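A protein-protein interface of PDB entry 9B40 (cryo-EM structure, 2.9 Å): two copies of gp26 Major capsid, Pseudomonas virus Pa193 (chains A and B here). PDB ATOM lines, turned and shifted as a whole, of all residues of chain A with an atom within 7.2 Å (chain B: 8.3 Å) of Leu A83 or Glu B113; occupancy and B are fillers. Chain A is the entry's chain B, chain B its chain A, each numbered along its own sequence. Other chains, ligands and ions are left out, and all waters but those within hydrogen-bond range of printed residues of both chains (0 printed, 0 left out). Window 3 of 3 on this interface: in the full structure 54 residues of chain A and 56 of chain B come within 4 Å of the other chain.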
ATOM      1  N   THR A  78      34.934 -17.361 -27.028  1.00  0.00           N
ATOM      2  CA  THR A  78      34.225 -16.522 -26.069  1.00  0.00           C
ATOM      3  C   THR A  78      33.477 -17.367 -25.039  1.00  0.00           C
ATOM      4  O   THR A  78      32.818 -18.348 -25.406  1.00  0.00           O
ATOM      5  CB  THR A  78      33.280 -15.569 -26.802  1.00  0.00           C
ATOM      6  OG1 THR A  78      32.664 -14.664 -25.875  1.00  0.00           O
ATOM      7  CG2 THR A  78      32.253 -16.306 -27.658  1.00  0.00           C
ATOM      8  N   PRO A  79      33.618 -17.067 -23.750  1.00  0.00           N
ATOM      9  CA  PRO A  79      32.864 -17.805 -22.734  1.00  0.00           C
ATOM     10  C   PRO A  79      31.406 -17.384 -22.691  1.00  0.00           C
ATOM     11  O   PRO A  79      31.034 -16.284 -23.107  1.00  0.00           O
ATOM     12  CB  PRO A  79      33.579 -17.451 -21.424  1.00  0.00           C
ATOM     13  CG  PRO A  79      34.862 -16.796 -21.819  1.00  0.00           C
ATOM     14  CD  PRO A  79      34.626 -16.178 -23.154  1.00  0.00           C
ATOM     15  N   ILE A  80      30.572 -18.289 -22.174  1.00  0.00           N
ATOM     16  CA  ILE A  80      29.162 -17.992 -21.953  1.00  0.00           C
ATOM     17  C   ILE A  80      28.986 -17.010 -20.794  1.00  0.00           C
ATOM     18  O   ILE A  80      27.887 -16.481 -20.587  1.00  0.00           O
ATOM     19  CB  ILE A  80      28.409 -19.322 -21.731  1.00  0.00           C
ATOM     20  CG1 ILE A  80      26.891 -19.137 -21.786  1.00  0.00           C
ATOM     21  CG2 ILE A  80      28.823 -19.953 -20.414  1.00  0.00           C
ATOM     22  CD1 ILE A  80      26.379 -18.777 -23.155  1.00  0.00           C
ATOM     23  N   GLN A  81      30.055 -16.765 -20.029  1.00  0.00           N
ATOM     24  CA  GLN A  81      30.045 -15.775 -18.954  1.00  0.00           C
ATOM     25  C   GLN A  81      29.627 -14.396 -19.451  1.00  0.00           C
ATOM     26  O   GLN A  81      28.740 -13.755 -18.877  1.00  0.00           O
ATOM     27  CB  GLN A  81      31.432 -15.717 -18.319  1.00  0.00           C
ATOM     28  CG  GLN A  81      31.566 -14.695 -17.226  1.00  0.00           C
ATOM     29  CD  GLN A  81      32.953 -14.667 -16.633  1.00  0.00           C
ATOM     30  OE1 GLN A  81      33.522 -13.601 -16.405  1.00  0.00           O
ATOM     31  NE2 GLN A  81      33.507 -15.844 -16.373  1.00  0.00           N
ATOM     32  N   PHE A  82      30.261 -13.923 -20.516  1.00  0.00           N
ATOM     33  CA  PHE A  82      29.853 -12.687 -21.170  1.00  0.00           C
ATOM     34  C   PHE A  82      28.717 -13.032 -22.123  1.00  0.00           C
ATOM     35  O   PHE A  82      28.143 -14.119 -22.035  1.00  0.00           O
ATOM     36  CB  PHE A  82      31.048 -12.037 -21.858  1.00  0.00           C
ATOM     37  CG  PHE A  82      32.265 -11.976 -20.991  1.00  0.00           C
ATOM     38  CD1 PHE A  82      32.419 -10.958 -20.070  1.00  0.00           C
ATOM     39  CD2 PHE A  82      33.248 -12.945 -21.084  1.00  0.00           C
ATOM     40  CE1 PHE A  82      33.530 -10.908 -19.261  1.00  0.00           C
ATOM     41  CE2 PHE A  82      34.360 -12.897 -20.281  1.00  0.00           C
ATOM     42  CZ  PHE A  82      34.503 -11.877 -19.369  1.00  0.00           C
ATOM     43  N   LEU A  83      28.372 -12.111 -23.033  1.00  0.00           N
ATOM     44  CA  LEU A  83      27.316 -12.307 -24.044  1.00  0.00           C
ATOM     45  C   LEU A  83      26.032 -12.876 -23.434  1.00  0.00           C
ATOM     46  O   LEU A  83      25.287 -13.626 -24.065  1.00  0.00           O
ATOM     47  CB  LEU A  83      27.832 -13.158 -25.216  1.00  0.00           C
ATOM     48  CG  LEU A  83      28.487 -14.546 -25.091  1.00  0.00           C
ATOM     49  CD1 LEU A  83      27.544 -15.695 -24.815  1.00  0.00           C
ATOM     50  CD2 LEU A  83      29.315 -14.831 -26.290  1.00  0.00           C
ATOM     51  N   GLN A  84      25.756 -12.466 -22.199  1.00  0.00           N
ATOM     52  CA  GLN A  84      24.716 -13.056 -21.358  1.00  0.00           C
ATOM     53  C   GLN A  84      24.048 -11.903 -20.618  1.00  0.00           C
ATOM     54  O   GLN A  84      24.598 -11.392 -19.639  1.00  0.00           O
ATOM     55  CB  GLN A  84      25.318 -14.066 -20.392  1.00  0.00           C
ATOM     56  CG  GLN A  84      24.479 -15.288 -20.106  1.00  0.00           C
ATOM     57  CD  GLN A  84      24.843 -15.912 -18.777  1.00  0.00           C
ATOM     58  OE1 GLN A  84      24.730 -15.278 -17.731  1.00  0.00           O
ATOM     59  NE2 GLN A  84      25.290 -17.159 -18.811  1.00  0.00           N
ATOM     60  N   THR A  85      22.874 -11.496 -21.085  1.00  0.00           N
ATOM     61  CA  THR A  85      22.190 -10.344 -20.517  1.00  0.00           C
ATOM     62  C   THR A  85      21.373 -10.776 -19.308  1.00  0.00           C
ATOM     63  O   THR A  85      20.588 -11.725 -19.386  1.00  0.00           O
ATOM     64  CB  THR A  85      21.289  -9.676 -21.553  1.00  0.00           C
ATOM     65  OG1 THR A  85      22.095  -9.113 -22.594  1.00  0.00           O
ATOM     66  CG2 THR A  85      20.468  -8.570 -20.908  1.00  0.00           C
ATOM     67  N   GLY B 110      18.252  -7.419 -23.760  1.00  0.00           N
ATOM     68  CA  GLY B 110      19.388  -8.117 -24.319  1.00  0.00           C
ATOM     69  C   GLY B 110      19.889  -7.492 -25.604  1.00  0.00           C
ATOM     70  O   GLY B 110      19.279  -6.593 -26.189  1.00  0.00           O
ATOM     71  N   SER B 111      21.038  -7.988 -26.049  1.00  0.00           N
ATOM     72  CA  SER B 111      21.653  -7.563 -27.294  1.00  0.00           C
ATOM     73  C   SER B 111      21.518  -8.662 -28.339  1.00  0.00           C
ATOM     74  O   SER B 111      21.325  -9.836 -28.016  1.00  0.00           O
ATOM     75  CB  SER B 111      23.130  -7.216 -27.087  1.00  0.00           C
ATOM     76  OG  SER B 111      23.706  -6.736 -28.287  1.00  0.00           O
ATOM     77  N   TRP B 112      21.621  -8.257 -29.606  1.00  0.00           N
ATOM     78  CA  TRP B 112      21.507  -9.211 -30.704  1.00  0.00           C
ATOM     79  C   TRP B 112      22.636 -10.234 -30.667  1.00  0.00           C
ATOM     80  O   TRP B 112      22.413 -11.424 -30.914  1.00  0.00           O
ATOM     81  CB  TRP B 112      21.500  -8.471 -32.040  1.00  0.00           C
ATOM     82  CG  TRP B 112      21.485  -9.381 -33.223  1.00  0.00           C
ATOM     83  CD1 TRP B 112      20.409 -10.041 -33.733  1.00  0.00           C
ATOM     84  CD2 TRP B 112      22.605  -9.749 -34.034  1.00  0.00           C
ATOM     85  NE1 TRP B 112      20.787 -10.790 -34.820  1.00  0.00           N
ATOM     86  CE2 TRP B 112      22.131 -10.628 -35.024  1.00  0.00           C
ATOM     87  CE3 TRP B 112      23.961  -9.417 -34.021  1.00  0.00           C
ATOM     88  CZ2 TRP B 112      22.964 -11.179 -35.990  1.00  0.00           C
ATOM     89  CZ3 TRP B 112      24.786  -9.965 -34.980  1.00  0.00           C
ATOM     90  CH2 TRP B 112      24.286 -10.836 -35.951  1.00  0.00           C
ATOM     91  N   GLU B 113      23.849  -9.792 -30.353  1.00  0.00           N
ATOM     92  CA  GLU B 113      25.019 -10.670 -30.325  1.00  0.00           C
ATOM     93  C   GLU B 113      25.211 -11.322 -28.956  1.00  0.00           C
ATOM     94  O   GLU B 113      26.301 -11.338 -28.388  1.00  0.00           O
ATOM     95  CB  GLU B 113      26.255  -9.884 -30.749  1.00  0.00           C
ATOM     96  CG  GLU B 113      26.506  -8.614 -29.947  1.00  0.00           C
ATOM     97  CD  GLU B 113      25.982  -7.375 -30.643  1.00  0.00           C
ATOM     98  OE1 GLU B 113      24.777  -7.082 -30.506  1.00  0.00           O
ATOM     99  OE2 GLU B 113      26.773  -6.696 -31.331  1.00  0.00           O
ATOM    100  N   ASP B 114      24.136 -11.898 -28.432  1.00  0.00           N
ATOM    101  CA  ASP B 114      24.146 -12.600 -27.160  1.00  0.00           C
ATOM    102  C   ASP B 114      23.712 -14.042 -27.375  1.00  0.00           C
ATOM    103  O   ASP B 114      23.232 -14.418 -28.446  1.00  0.00           O
ATOM    104  CB  ASP B 114      23.222 -11.920 -26.142  1.00  0.00           C
ATOM    105  CG  ASP B 114      23.897 -10.785 -25.407  1.00  0.00           C
ATOM    106  OD1 ASP B 114      25.000 -10.378 -25.822  1.00  0.00           O
ATOM    107  OD2 ASP B 114      23.322 -10.295 -24.414  1.00  0.00           O
ATOM    108  N   GLN B 115      23.880 -14.852 -26.340  1.00  0.00           N
ATOM    109  CA  GLN B 115      23.438 -16.237 -26.389  1.00  0.00           C
ATOM    110  C   GLN B 115      22.340 -16.550 -25.390  1.00  0.00           C
ATOM    111  O   GLN B 115      21.430 -17.307 -25.715  1.00  0.00           O
ATOM    112  CB  GLN B 115      24.619 -17.189 -26.153  1.00  0.00           C
ATOM    113  CG  GLN B 115      24.339 -18.661 -26.425  1.00  0.00           C
ATOM    114  CD  GLN B 115      24.385 -19.012 -27.900  1.00  0.00           C
ATOM    115  OE1 GLN B 115      25.387 -19.527 -28.394  1.00  0.00           O
ATOM    116  NE2 GLN B 115      23.293 -18.750 -28.608  1.00  0.00           N
ATOM    117  N   GLU B 116      22.384 -15.974 -24.189  1.00  0.00           N
ATOM    118  CA  GLU B 116      21.445 -16.338 -23.138  1.00  0.00           C
ATOM    119  C   GLU B 116      20.948 -15.097 -22.410  1.00  0.00           C
ATOM    120  O   GLU B 116      21.594 -14.047 -22.400  1.00  0.00           O
ATOM    121  CB  GLU B 116      22.076 -17.305 -22.127  1.00  0.00           C
ATOM    122  CG  GLU B 116      22.063 -18.760 -22.558  1.00  0.00           C
ATOM    123  CD  GLU B 116      22.682 -19.676 -21.523  1.00  0.00           C
ATOM    124  OE1 GLU B 116      22.913 -19.215 -20.386  1.00  0.00           O
ATOM    125  OE2 GLU B 116      22.939 -20.856 -21.844  1.00  0.00           O
ATOM    126  N   ILE B 117      19.776 -15.245 -21.801  1.00  0.00           N
ATOM    127  CA  ILE B 117      19.178 -14.258 -20.910  1.00  0.00           C
ATOM    128  C   ILE B 117      18.882 -14.933 -19.579  1.00  0.00           C
ATOM    129  O   ILE B 117      18.321 -16.034 -19.546  1.00  0.00           O
ATOM    130  CB  ILE B 117      17.903 -13.639 -21.512  1.00  0.00           C
ATOM    131  CG1 ILE B 117      18.267 -12.620 -22.593  1.00  0.00           C
ATOM    132  CG2 ILE B 117      17.001 -13.060 -20.436  1.00  0.00           C
ATOM    133  CD1 ILE B 117      17.163 -11.645 -22.898  1.00  0.00           C
ATOM    134  N   VAL B 118      19.262 -14.273 -18.486  1.00  0.00           N
ATOM    135  CA  VAL B 118      19.135 -14.814 -17.139  1.00  0.00           C
ATOM    136  C   VAL B 118      18.148 -13.961 -16.355  1.00  0.00           C
ATOM    137  O   VAL B 118      18.221 -12.727 -16.387  1.00  0.00           O
ATOM    138  CB  VAL B 118      20.495 -14.866 -16.425  1.00  0.00           C
ATOM    139  CG1 VAL B 118      20.369 -15.604 -15.110  1.00  0.00           C
ATOM    140  CG2 VAL B 118      21.523 -15.529 -17.315  1.00  0.00           C
ATOM    141  N   ARG B 148      18.088 -19.502 -16.920  1.00  0.00           N
ATOM    142  CA  ARG B 148      18.728 -19.112 -18.167  1.00  0.00           C
ATOM    143  C   ARG B 148      17.908 -19.613 -19.349  1.00  0.00           C
ATOM    144  O   ARG B 148      17.336 -20.708 -19.306  1.00  0.00           O
ATOM    145  CB  ARG B 148      20.166 -19.646 -18.229  1.00  0.00           C
ATOM    146  CG  ARG B 148      20.280 -21.156 -18.374  1.00  0.00           C
ATOM    147  CD  ARG B 148      21.655 -21.681 -17.993  1.00  0.00           C
ATOM    148  NE  ARG B 148      22.744 -20.790 -18.371  1.00  0.00           N
ATOM    149  CZ  ARG B 148      24.027 -21.075 -18.195  1.00  0.00           C
ATOM    150  NH1 ARG B 148      24.412 -22.210 -17.638  1.00  0.00           N
ATOM    151  NH2 ARG B 148      24.946 -20.197 -18.586  1.00  0.00           N
ATOM    152  N   ARG B 149      17.806 -18.779 -20.382  1.00  0.00           N
ATOM    153  CA  ARG B 149      17.110 -19.122 -21.617  1.00  0.00           C
ATOM    154  C   ARG B 149      17.949 -18.659 -22.794  1.00  0.00           C
ATOM    155  O   ARG B 149      18.350 -17.494 -22.845  1.00  0.00           O
ATOM    156  CB  ARG B 149      15.725 -18.477 -21.675  1.00  0.00           C
ATOM    157  CG  ARG B 149      14.811 -18.923 -20.567  1.00  0.00           C
ATOM    158  CD  ARG B 149      14.304 -20.317 -20.837  1.00  0.00           C
ATOM    159  NE  ARG B 149      12.876 -20.397 -20.580  1.00  0.00           N
ATOM    160  CZ  ARG B 149      12.354 -20.836 -19.445  1.00  0.00           C
ATOM    161  NH1 ARG B 149      13.112 -21.333 -18.483  1.00  0.00           N
ATOM    162  NH2 ARG B 149      11.040 -20.778 -19.271  1.00  0.00           N
ATOM    163  N   ILE B 151      19.070 -17.800 -26.830  1.00  0.00           N
ATOM    164  CA  ILE B 151      18.583 -16.800 -27.771  1.00  0.00           C
ATOM    165  C   ILE B 151      18.655 -17.368 -29.180  1.00  0.00           C
ATOM    166  O   ILE B 151      19.678 -17.933 -29.580  1.00  0.00           O
ATOM    167  CB  ILE B 151      19.390 -15.490 -27.653  1.00  0.00           C
ATOM    168  CG1 ILE B 151      19.001 -14.746 -26.375  1.00  0.00           C
ATOM    169  CG2 ILE B 151      19.198 -14.602 -28.870  1.00  0.00           C
ATOM    170  CD1 ILE B 151      19.969 -13.665 -25.986  1.00  0.00           C
ATOM    171  N   ARG B 153      18.370 -16.483 -33.213  1.00  0.00           N
ATOM    172  CA  ARG B 153      18.500 -15.410 -34.190  1.00  0.00           C
ATOM    173  C   ARG B 153      17.963 -15.894 -35.527  1.00  0.00           C
ATOM    174  O   ARG B 153      18.467 -16.875 -36.085  1.00  0.00           O
ATOM    175  CB  ARG B 153      19.956 -14.968 -34.331  1.00  0.00           C
ATOM    176  CG  ARG B 153      20.401 -13.930 -33.322  1.00  0.00           C
ATOM    177  CD  ARG B 153      21.910 -13.765 -33.343  1.00  0.00           C
ATOM    178  NE  ARG B 153      22.595 -15.028 -33.102  1.00  0.00           N
ATOM    179  CZ  ARG B 153      22.818 -15.543 -31.902  1.00  0.00           C
ATOM    180  NH1 ARG B 153      22.438 -14.917 -30.801  1.00  0.00           N
ATOM    181  NH2 ARG B 153      23.440 -16.713 -31.803  1.00  0.00           N
ATOM    182  N   GLN B 342      15.202  -9.571 -28.300  1.00  0.00           N
ATOM    183  CA  GLN B 342      16.380  -8.712 -28.331  1.00  0.00           C
ATOM    184  C   GLN B 342      16.168  -7.553 -29.290  1.00  0.00           C
ATOM    185  O   GLN B 342      16.524  -6.410 -28.982  1.00  0.00           O
ATOM    186  CB  GLN B 342      17.638  -9.492 -28.730  1.00  0.00           C
ATOM    187  CG  GLN B 342      18.191 -10.524 -27.735  1.00  0.00           C
ATOM    188  CD  GLN B 342      17.172 -11.511 -27.228  1.00  0.00           C
ATOM    189  OE1 GLN B 342      16.953 -11.640 -26.033  1.00  0.00           O
ATOM    190  NE2 GLN B 342      16.549 -12.228 -28.144  1.00  0.00           N
ATOM    191  N   SER B 343      15.574  -7.831 -30.448  1.00  0.00           N
ATOM    192  CA  SER B 343      15.362  -6.819 -31.470  1.00  0.00           C
ATOM    193  C   SER B 343      14.339  -7.338 -32.466  1.00  0.00           C
ATOM    194  O   SER B 343      14.445  -8.478 -32.928  1.00  0.00           O
ATOM    195  CB  SER B 343      16.670  -6.480 -32.177  1.00  0.00           C
ATOM    196  OG  SER B 343      17.301  -7.651 -32.661  1.00  0.00           O
ATOM    197  N   ILE B 346      16.600  -5.709 -37.349  1.00  0.00           N
ATOM    198  CA  ILE B 346      17.837  -4.959 -37.541  1.00  0.00           C
ATOM    199  C   ILE B 346      18.314  -5.179 -38.967  1.00  0.00           C
ATOM    200  O   ILE B 346      18.099  -6.247 -39.547  1.00  0.00           O
ATOM    201  CB  ILE B 346      18.945  -5.336 -36.527  1.00  0.00           C
ATOM    202  CG1 ILE B 346      19.744  -6.565 -36.973  1.00  0.00           C
ATOM    203  CG2 ILE B 346      18.369  -5.548 -35.153  1.00  0.00           C
ATOM    204  CD1 ILE B 346      20.686  -7.104 -35.927  1.00  0.00           C
ATOM    205  N   GLY B 364      16.144 -11.244 -33.181  1.00  0.00           N
ATOM    206  CA  GLY B 364      16.470 -12.144 -32.094  1.00  0.00           C
ATOM    207  C   GLY B 364      15.315 -12.273 -31.125  1.00  0.00           C
ATOM    208  O   GLY B 364      14.597 -11.314 -30.848  1.00  0.00           O
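CD1 of Ile A80 touches CB of Gln B115, at 3.8 Å.
Leu A83 touches Glu B113.
Asp B114 touches Leu A83 (CB to O, 3.4 Å).
Glu B116 touches Leu A83 (N to O, 3.7 Å).
Gln A84 touches Asp B114.
Glu B116 touches Gln A84.
Gln A84 touches Val B118.
Thr A85 touches Gly B110 (OG1 to CA, 3.4 Å).
Thr A85 touches Ser B111 (OG1 to N, 3.8 Å).
Ile B117 touches Thr A85 (CA to O, 3.3 Å).
No position is printed for both chains.
Of the 16 pairs that touch across the chains among the printed residues, none has its exchanged pair printed and touching as well.
Of the 17 printed residues of chain B, 9 touch a printed residue of chain A.
Hydrophobic or aromatic side chains of chain B that line the printed part of chain A: Ile B117 and Val B118.
Printed residues of chain A that touch a printed residue of chain B: Ile A80, Leu A83, Gln A84 and Thr A85.
Hydrophobic or aromatic side chains of chain A that line the printed part of chain B: Ile A80 and Leu A83.
Among the printed residues, 16 pairs touch across the chains.
Among the printed residues, no Asp or Glu carboxylate lies within 4 Å of a Lys or Arg side-chain nitrogen of the other chain.
Leu A83 touches just these residues of chain B: Glu B113 (3.96 Å), Asp B114 (3.4 Å), Gln B115 (2.9 Å) and Glu B116 (3.7 Å).
Of the printed residues of chain A, Glu B113 touches Leu A83.
Of the printed residues of chain A, Ser B111 touches Thr A85.
Printed residues of chain A within 4 Å of Gly B110: Thr A85.
OD2 of Asp B114 sits at hydrogen-bond distance from OG1 of Thr A85 (2.5 Å).
NH2 of Arg B148 sits close to NE2 of Gln A84 (3.1 Å).
The backbone carbonyl oxygen (O) of Glu B116 sits at hydrogen-bond distance from the backbone NH (N) of Thr A85 (3.1 Å).
N of Val B118 lies within hydrogen-bond range of O of Thr A85 (3.0 Å).
N of Gln B115 lies within hydrogen-bond range of O of Leu A83 (2.9 Å).
The backbone carbonyl oxygen (O) of Ile A80 lies within hydrogen-bond range of the side-chain amide nitrogen (NE2) of Gln A84 (3.2 Å).
O of Asp B114 sits at hydrogen-bond distance from NH1 of Arg B153.
The backbone NH (N) of Ile B151 sits at hydrogen-bond distance from the backbone carbonyl oxygen (O) of Gln B115, 2.7 Å away.
N of Ile B117 is in hydrogen-bond range of O of Arg B149 (2.9 Å).
OG of Ser B111 lies within hydrogen-bond range of OE1 of Glu B113 (2.5 Å).
The guanidinium group (NE) of Arg B148 is in salt-bridge range of the side-chain carboxylate (OE1) of Glu B116 (2.6 Å).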
